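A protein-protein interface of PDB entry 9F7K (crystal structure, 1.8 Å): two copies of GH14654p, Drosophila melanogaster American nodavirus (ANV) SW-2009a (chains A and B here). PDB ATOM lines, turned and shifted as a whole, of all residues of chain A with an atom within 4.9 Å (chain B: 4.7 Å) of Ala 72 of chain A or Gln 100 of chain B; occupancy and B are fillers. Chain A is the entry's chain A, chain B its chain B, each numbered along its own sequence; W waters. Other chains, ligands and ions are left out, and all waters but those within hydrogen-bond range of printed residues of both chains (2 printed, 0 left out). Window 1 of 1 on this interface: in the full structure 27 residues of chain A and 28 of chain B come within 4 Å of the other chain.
Among the printed residues, pairs that only touch across the chains: His 71 of chain A with Phe 103 of chain B (3.5 Å), Asp 69 of chain A with Phe 103 of chain B (3.5 Å), Ile 67 of chain A with Ala 96 of chain B (3.7 Å), Trp 68 of chain A with Arg 101 of chain B (3.7 Å), Trp 68 of chain A with Phe 146 of chain B (3.8 Å), Gln 54 of chain A with Phe 104 of chain B (3.8 Å), Ala 72 of chain A with Gln 100 of chain B (3.8 Å), Ala 72 of chain A with Ala 96 of chain B (3.9 Å) and Gln 54 of chain A with Phe 146 of chain B (3.9 Å).
Water W2 bridges O of Ala 72 of chain A (2.8 Å) and ND2 of Asn 99 of chain B (2.9 Å).
Water W1 lies within hydrogen-bond range of OE1 of Gln 54 of chain A (2.9 Å), OD2 of Asp 69 of chain A (2.9 Å) and NE2 of Gln 100 of chain B (3.1 Å).
Of the 11 printed residues of chain A, 6 touch a printed residue of chain B.
Along chain A the printed residues that touch a printed residue of chain B span positions 54 to 72.
Of the 10 printed residues of chain B, 6 touch a printed residue of chain A.
Printed residues of chain B that touch a printed residue of chain A: Ala 96, Gln 100, Arg 101, Phe 103, Phe 104 and Phe 146.
Among the printed residues, 11 pairs touch across the chains.
Among the printed residues, no Asp or Glu carboxylate lies within 4 Å of a Lys or Arg side-chain nitrogen of the other chain.
No position is printed for both chains.
Of the printed residues of chain B, Trp 68 of chain A touches Gln 100, Arg 101 and Phe 146.
Of the printed residues of chain B, His 71 of chain A touches Phe 103.
Ala 72 of chain A touches just these residues of chain B: Ala 96 and Gln 100.
Of the printed residues of chain A, Ala 96 of chain B touches Ile 67 (3.7 Å) and Ala 72 (3.9 Å).
Of the printed residues of chain A, Gln 100 of chain B touches Gln 54 (3.5 Å), Trp 68 (3.2 Å) and Ala 72 (3.8 Å).
Printed residues of chain A within 4 Å of Arg 101 of chain B: Trp 68.
The nearest residue of chain B that does not touch Ala 72 of chain A is Asn 99 of chain B (4.03 Å).
The nearest printed residue of chain A that does not touch Gln 100 of chain B is Asp 69 of chain A (4.001 Å).
The side-chain amide oxygen of Gln 54 of chain A sits at hydrogen-bond distance from the indole nitrogen of Trp 68 of chain A, 2.9 Å away.
The side-chain carboxylate of Asp 69 of chain A lies within hydrogen-bond range of a ring nitrogen (ND1) of His 71 of chain A (2.8 Å).
OE1 of Gln 100 of chain B lies within hydrogen-bond range of NH1 of Arg 101 of chain B (2.7 Å).
The side-chain amide nitrogen of Gln 100 of chain B sits at hydrogen-bond distance from the side-chain amide oxygen of Gln 54 of chain A, at 3.5 Å.
The side-chain amide nitrogen (NE2) of Gln 100 of chain B sits close to the indole nitrogen (NE1) of Trp 68 of chain A (3.2 Å).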
ATOM      1  N   GLN A  54       5.348  14.828  16.556  1.00  0.00           N
ATOM      2  CA  GLN A  54       6.727  14.611  16.147  1.00  0.00           C
ATOM      3  C   GLN A  54       7.577  14.037  17.293  1.00  0.00           C
ATOM      4  O   GLN A  54       8.737  13.689  17.067  1.00  0.00           O
ATOM      5  CB  GLN A  54       7.373  15.930  15.662  1.00  0.00           C
ATOM      6  CG  GLN A  54       8.527  15.721  14.696  1.00  0.00           C
ATOM      7  CD  GLN A  54       9.147  16.991  14.129  1.00  0.00           C
ATOM      8  OE1 GLN A  54       8.531  18.044  14.087  1.00  0.00           O
ATOM      9  NE2 GLN A  54      10.412  16.900  13.735  1.00  0.00           N
ATOM     10  N   ILE A  67       2.872  24.481  20.795  1.00  0.00           N
ATOM     11  CA  ILE A  67       3.647  24.713  19.584  1.00  0.00           C
ATOM     12  C   ILE A  67       4.959  23.954  19.707  1.00  0.00           C
ATOM     13  O   ILE A  67       5.530  23.856  20.789  1.00  0.00           O
ATOM     14  CB  ILE A  67       3.977  26.213  19.479  1.00  0.00           C
ATOM     15  CG1 ILE A  67       2.719  27.046  19.277  1.00  0.00           C
ATOM     16  CG2 ILE A  67       4.994  26.466  18.367  1.00  0.00           C
ATOM     17  CD1 ILE A  67       3.041  28.545  19.483  1.00  0.00           C
ATOM     18  N   TRP A  68       5.485  23.470  18.582  1.00  0.00           N
ATOM     19  CA  TRP A  68       6.805  22.871  18.659  1.00  0.00           C
ATOM     20  C   TRP A  68       7.648  23.325  17.468  1.00  0.00           C
ATOM     21  O   TRP A  68       7.177  24.103  16.627  1.00  0.00           O
ATOM     22  CB  TRP A  68       6.714  21.365  18.821  1.00  0.00           C
ATOM     23  CG  TRP A  68       6.384  20.590  17.592  1.00  0.00           C
ATOM     24  CD1 TRP A  68       7.250  20.047  16.691  1.00  0.00           C
ATOM     25  CD2 TRP A  68       5.057  20.226  17.145  1.00  0.00           C
ATOM     26  NE1 TRP A  68       6.560  19.397  15.701  1.00  0.00           N
ATOM     27  CE2 TRP A  68       5.218  19.478  15.952  1.00  0.00           C
ATOM     28  CE3 TRP A  68       3.763  20.448  17.637  1.00  0.00           C
ATOM     29  CZ2 TRP A  68       4.141  18.955  15.250  1.00  0.00           C
ATOM     30  CZ3 TRP A  68       2.689  19.921  16.932  1.00  0.00           C
ATOM     31  CH2 TRP A  68       2.874  19.209  15.742  1.00  0.00           C
ATOM     32  N   ASP A  69       8.909  22.874  17.470  1.00  0.00           N
ATOM     33  CA  ASP A  69      10.002  23.321  16.611  1.00  0.00           C
ATOM     34  C   ASP A  69      10.584  24.624  17.165  1.00  0.00           C
ATOM     35  O   ASP A  69       9.907  25.647  17.193  1.00  0.00           O
ATOM     36  CB  ASP A  69       9.662  23.481  15.114  1.00  0.00           C
ATOM     37  CG  ASP A  69      10.921  23.640  14.284  1.00  0.00           C
ATOM     38  OD1 ASP A  69      11.494  24.756  14.257  1.00  0.00           O
ATOM     39  OD2 ASP A  69      11.364  22.609  13.697  1.00  0.00           O
ATOM     40  N   SER A  70      11.845  24.582  17.562  1.00  0.00           N
ATOM     41  CA  SER A  70      12.513  25.731  18.185  1.00  0.00           C
ATOM     42  C   SER A  70      12.384  27.011  17.364  1.00  0.00           C
ATOM     43  O   SER A  70      12.281  28.091  17.955  1.00  0.00           O
ATOM     44  CB  SER A  70      13.988  25.433  18.440  1.00  0.00           C
ATOM     45  OG  SER A  70      14.675  25.166  17.228  1.00  0.00           O
ATOM     46  N   HIS A  71      12.479  26.920  16.029  1.00  0.00           N
ATOM     47  CA  HIS A  71      12.432  28.087  15.157  1.00  0.00           C
ATOM     48  C   HIS A  71      11.030  28.701  15.219  1.00  0.00           C
ATOM     49  O   HIS A  71      10.890  29.931  15.355  1.00  0.00           O
ATOM     50  CB  HIS A  71      12.797  27.731  13.708  1.00  0.00           C
ATOM     51  CG  HIS A  71      14.102  26.963  13.565  1.00  0.00           C
ATOM     52  ND1 HIS A  71      14.051  25.567  13.549  1.00  0.00           N
ATOM     53  CD2 HIS A  71      15.373  27.310  13.517  1.00  0.00           C
ATOM     54  CE1 HIS A  71      15.315  25.110  13.464  1.00  0.00           C
ATOM     55  NE2 HIS A  71      16.148  26.132  13.460  1.00  0.00           N
ATOM     56  N   ALA A  72      10.025  27.856  15.114  1.00  0.00           N
ATOM     57  CA  ALA A  72       8.635  28.315  15.104  1.00  0.00           C
ATOM     58  C   ALA A  72       8.270  28.896  16.485  1.00  0.00           C
ATOM     59  O   ALA A  72       7.625  29.963  16.577  1.00  0.00           O
ATOM     60  CB  ALA A  72       7.711  27.199  14.789  1.00  0.00           C
ATOM     61  N   ILE A  73       8.769  28.242  17.541  1.00  0.00           N
ATOM     62  CA  ILE A  73       8.534  28.740  18.895  1.00  0.00           C
ATOM     63  C   ILE A  73       9.151  30.108  19.114  1.00  0.00           C
ATOM     64  O   ILE A  73       8.494  31.018  19.654  1.00  0.00           O
ATOM     65  CB  ILE A  73       9.024  27.760  19.959  1.00  0.00           C
ATOM     66  CG1 ILE A  73       8.253  26.461  19.973  1.00  0.00           C
ATOM     67  CG2 ILE A  73       9.007  28.391  21.375  1.00  0.00           C
ATOM     68  CD1 ILE A  73       8.999  25.351  20.708  1.00  0.00           C
ATOM     69  N   ALA A  74      10.405  30.267  18.689  1.00  0.00           N
ATOM     70  CA  ALA A  74      11.112  31.512  18.911  1.00  0.00           C
ATOM     71  C   ALA A  74      10.437  32.658  18.143  1.00  0.00           C
ATOM     72  O   ALA A  74      10.254  33.740  18.736  1.00  0.00           O
ATOM     73  CB  ALA A  74      12.553  31.346  18.541  1.00  0.00           C
ATOM     74  N   ALA A  75      10.056  32.406  16.885  1.00  0.00           N
ATOM     75  CA  ALA A  75       9.367  33.417  16.065  1.00  0.00           C
ATOM     76  C   ALA A  75       8.003  33.804  16.681  1.00  0.00           C
ATOM     77  O   ALA A  75       7.669  34.991  16.762  1.00  0.00           O
ATOM     78  CB  ALA A  75       9.206  32.917  14.657  1.00  0.00           C
ATOM     79  N   TYR A  76       7.266  32.828  17.197  1.00  0.00           N
ATOM     80  CA  TYR A  76       6.025  33.096  17.888  1.00  0.00           C
ATOM     81  C   TYR A  76       6.241  33.972  19.126  1.00  0.00           C
ATOM     82  O   TYR A  76       5.505  34.965  19.344  1.00  0.00           O
ATOM     83  CB  TYR A  76       5.412  31.749  18.224  1.00  0.00           C
ATOM     84  CG  TYR A  76       4.202  31.823  19.151  1.00  0.00           C
ATOM     85  CD1 TYR A  76       2.912  31.930  18.632  1.00  0.00           C
ATOM     86  CD2 TYR A  76       4.339  31.797  20.554  1.00  0.00           C
ATOM     87  CE1 TYR A  76       1.789  31.959  19.451  1.00  0.00           C
ATOM     88  CE2 TYR A  76       3.227  31.887  21.381  1.00  0.00           C
ATOM     89  CZ  TYR A  76       1.947  31.962  20.831  1.00  0.00           C
ATOM     90  OH  TYR A  76       0.826  31.914  21.658  1.00  0.00           O
ATOM     91  N   ALA B  96       2.253  29.779  13.685  1.00  0.00           N
ATOM     92  CA  ALA B  96       3.216  28.880  14.296  1.00  0.00           C
ATOM     93  C   ALA B  96       3.051  27.449  13.779  1.00  0.00           C
ATOM     94  O   ALA B  96       4.047  26.737  13.662  1.00  0.00           O
ATOM     95  CB  ALA B  96       3.176  28.951  15.803  1.00  0.00           C
ATOM     96  N   ILE B  97       1.839  27.029  13.459  1.00  0.00           N
ATOM     97  CA  ILE B  97       1.592  25.697  12.910  1.00  0.00           C
ATOM     98  C   ILE B  97       2.141  25.624  11.485  1.00  0.00           C
ATOM     99  O   ILE B  97       2.871  24.697  11.148  1.00  0.00           O
ATOM    100  CB  ILE B  97       0.098  25.343  12.945  1.00  0.00           C
ATOM    101  CG1 ILE B  97      -0.436  25.226  14.369  1.00  0.00           C
ATOM    102  CG2 ILE B  97      -0.181  24.111  12.084  1.00  0.00           C
ATOM    103  CD1 ILE B  97      -1.952  25.163  14.383  1.00  0.00           C
ATOM    104  N   VAL B  98       1.865  26.649  10.667  1.00  0.00           N
ATOM    105  CA  VAL B  98       2.364  26.668   9.313  1.00  0.00           C
ATOM    106  C   VAL B  98       3.911  26.750   9.322  1.00  0.00           C
ATOM    107  O   VAL B  98       4.546  25.992   8.609  1.00  0.00           O
ATOM    108  CB  VAL B  98       1.723  27.778   8.453  1.00  0.00           C
ATOM    109  CG1 VAL B  98       2.406  27.858   7.095  1.00  0.00           C
ATOM    110  CG2 VAL B  98       0.225  27.570   8.287  1.00  0.00           C
ATOM    111  N   ASN B  99       4.500  27.587  10.192  1.00  0.00           N
ATOM    112  CA  ASN B  99       5.939  27.665  10.332  1.00  0.00           C
ATOM    113  C   ASN B  99       6.534  26.322  10.755  1.00  0.00           C
ATOM    114  O   ASN B  99       7.565  25.922  10.192  1.00  0.00           O
ATOM    115  CB  ASN B  99       6.330  28.752  11.335  1.00  0.00           C
ATOM    116  CG  ASN B  99       6.377  30.121  10.709  1.00  0.00           C
ATOM    117  OD1 ASN B  99       6.342  30.311   9.480  1.00  0.00           O
ATOM    118  ND2 ASN B  99       6.434  31.109  11.587  1.00  0.00           N
ATOM    119  N   GLN B 100       5.951  25.670  11.759  1.00  0.00           N
ATOM    120  CA  GLN B 100       6.435  24.352  12.172  1.00  0.00           C
ATOM    121  C   GLN B 100       6.509  23.428  10.948  1.00  0.00           C
ATOM    122  O   GLN B 100       7.502  22.684  10.774  1.00  0.00           O
ATOM    123  CB  GLN B 100       5.611  23.780  13.328  1.00  0.00           C
ATOM    124  CG  GLN B 100       6.057  22.384  13.769  1.00  0.00           C
ATOM    125  CD  GLN B 100       5.488  21.270  12.903  1.00  0.00           C
ATOM    126  OE1 GLN B 100       4.327  21.279  12.514  1.00  0.00           O
ATOM    127  NE2 GLN B 100       6.304  20.278  12.596  1.00  0.00           N
ATOM    128  N   ARG B 101       5.426  23.383  10.168  1.00  0.00           N
ATOM    129  CA  ARG B 101       5.414  22.538   8.970  1.00  0.00           C
ATOM    130  C   ARG B 101       6.549  22.910   8.001  1.00  0.00           C
ATOM    131  O   ARG B 101       7.174  22.031   7.408  1.00  0.00           O
ATOM    132  CB  ARG B 101       4.050  22.547   8.283  1.00  0.00           C
ATOM    133  CG  ARG B 101       2.887  22.015   9.121  1.00  0.00           C
ATOM    134  CD  ARG B 101       3.034  20.564   9.514  1.00  0.00           C
ATOM    135  NE  ARG B 101       1.723  20.078   9.902  1.00  0.00           N
ATOM    136  CZ  ARG B 101       1.271  19.735  11.095  1.00  0.00           C
ATOM    137  NH1 ARG B 101       2.026  19.829  12.170  1.00  0.00           N
ATOM    138  NH2 ARG B 101       0.026  19.277  11.185  1.00  0.00           N
ATOM    139  N   LEU B 102       6.776  24.205   7.748  1.00  0.00           N
ATOM    140  CA  LEU B 102       7.853  24.640   6.876  1.00  0.00           C
ATOM    141  C   LEU B 102       9.222  24.193   7.432  1.00  0.00           C
ATOM    142  O   LEU B 102      10.066  23.762   6.635  1.00  0.00           O
ATOM    143  CB  LEU B 102       7.815  26.156   6.711  1.00  0.00           C
ATOM    144  CG  LEU B 102       6.551  26.731   6.040  1.00  0.00           C
ATOM    145  CD1 LEU B 102       6.533  28.246   6.071  1.00  0.00           C
ATOM    146  CD2 LEU B 102       6.445  26.263   4.599  1.00  0.00           C
ATOM    147  N   PHE B 103       9.463  24.375   8.754  1.00  0.00           N
ATOM    148  CA  PHE B 103      10.739  23.947   9.351  1.00  0.00           C
ATOM    149  C   PHE B 103      10.905  22.414   9.322  1.00  0.00           C
ATOM    150  O   PHE B 103      12.036  21.921   9.212  1.00  0.00           O
ATOM    151  CB  PHE B 103      10.915  24.506  10.770  1.00  0.00           C
ATOM    152  CG  PHE B 103      11.245  25.979  10.730  1.00  0.00           C
ATOM    153  CD1 PHE B 103      12.498  26.403  10.315  1.00  0.00           C
ATOM    154  CD2 PHE B 103      10.314  26.939  11.073  1.00  0.00           C
ATOM    155  CE1 PHE B 103      12.808  27.757  10.208  1.00  0.00           C
ATOM    156  CE2 PHE B 103      10.643  28.291  11.027  1.00  0.00           C
ATOM    157  CZ  PHE B 103      11.858  28.707  10.527  1.00  0.00           C
ATOM    158  N   PHE B 104       9.793  21.694   9.390  1.00  0.00           N
ATOM    159  CA  PHE B 104       9.762  20.232   9.228  1.00  0.00           C
ATOM    160  C   PHE B 104      10.125  19.818   7.803  1.00  0.00           C
ATOM    161  O   PHE B 104      10.936  18.916   7.578  1.00  0.00           O
ATOM    162  CB  PHE B 104       8.386  19.659   9.556  1.00  0.00           C
ATOM    163  CG  PHE B 104       8.295  18.150   9.362  1.00  0.00           C
ATOM    164  CD1 PHE B 104       8.847  17.283  10.291  1.00  0.00           C
ATOM    165  CD2 PHE B 104       7.622  17.646   8.277  1.00  0.00           C
ATOM    166  CE1 PHE B 104       8.740  15.910  10.113  1.00  0.00           C
ATOM    167  CE2 PHE B 104       7.504  16.269   8.121  1.00  0.00           C
ATOM    168  CZ  PHE B 104       8.061  15.432   9.035  1.00  0.00           C
ATOM    169  N   PHE B 146       1.111  13.708  10.824  1.00  0.00           N
ATOM    170  CA  PHE B 146       0.670  15.089  10.789  1.00  0.00           C
ATOM    171  C   PHE B 146      -0.634  15.258  10.022  1.00  0.00           C
ATOM    172  O   PHE B 146      -1.411  16.172  10.295  1.00  0.00           O
ATOM    173  CB  PHE B 146       1.733  15.977  10.131  1.00  0.00           C
ATOM    174  CG  PHE B 146       2.998  16.173  10.919  1.00  0.00           C
ATOM    175  CD1 PHE B 146       3.123  15.735  12.234  1.00  0.00           C
ATOM    176  CD2 PHE B 146       4.096  16.781  10.322  1.00  0.00           C
ATOM    177  CE1 PHE B 146       4.307  15.942  12.939  1.00  0.00           C
ATOM    178  CE2 PHE B 146       5.268  16.961  11.027  1.00  0.00           C
ATOM    179  CZ  PHE B 146       5.394  16.515  12.306  1.00  0.00           C
HETATM  180  O   HOH W   1       9.356  20.569  12.990  1.00  0.00           O
HETATM  181  O   HOH W   2       6.009  30.712  14.414  1.00  0.00           O
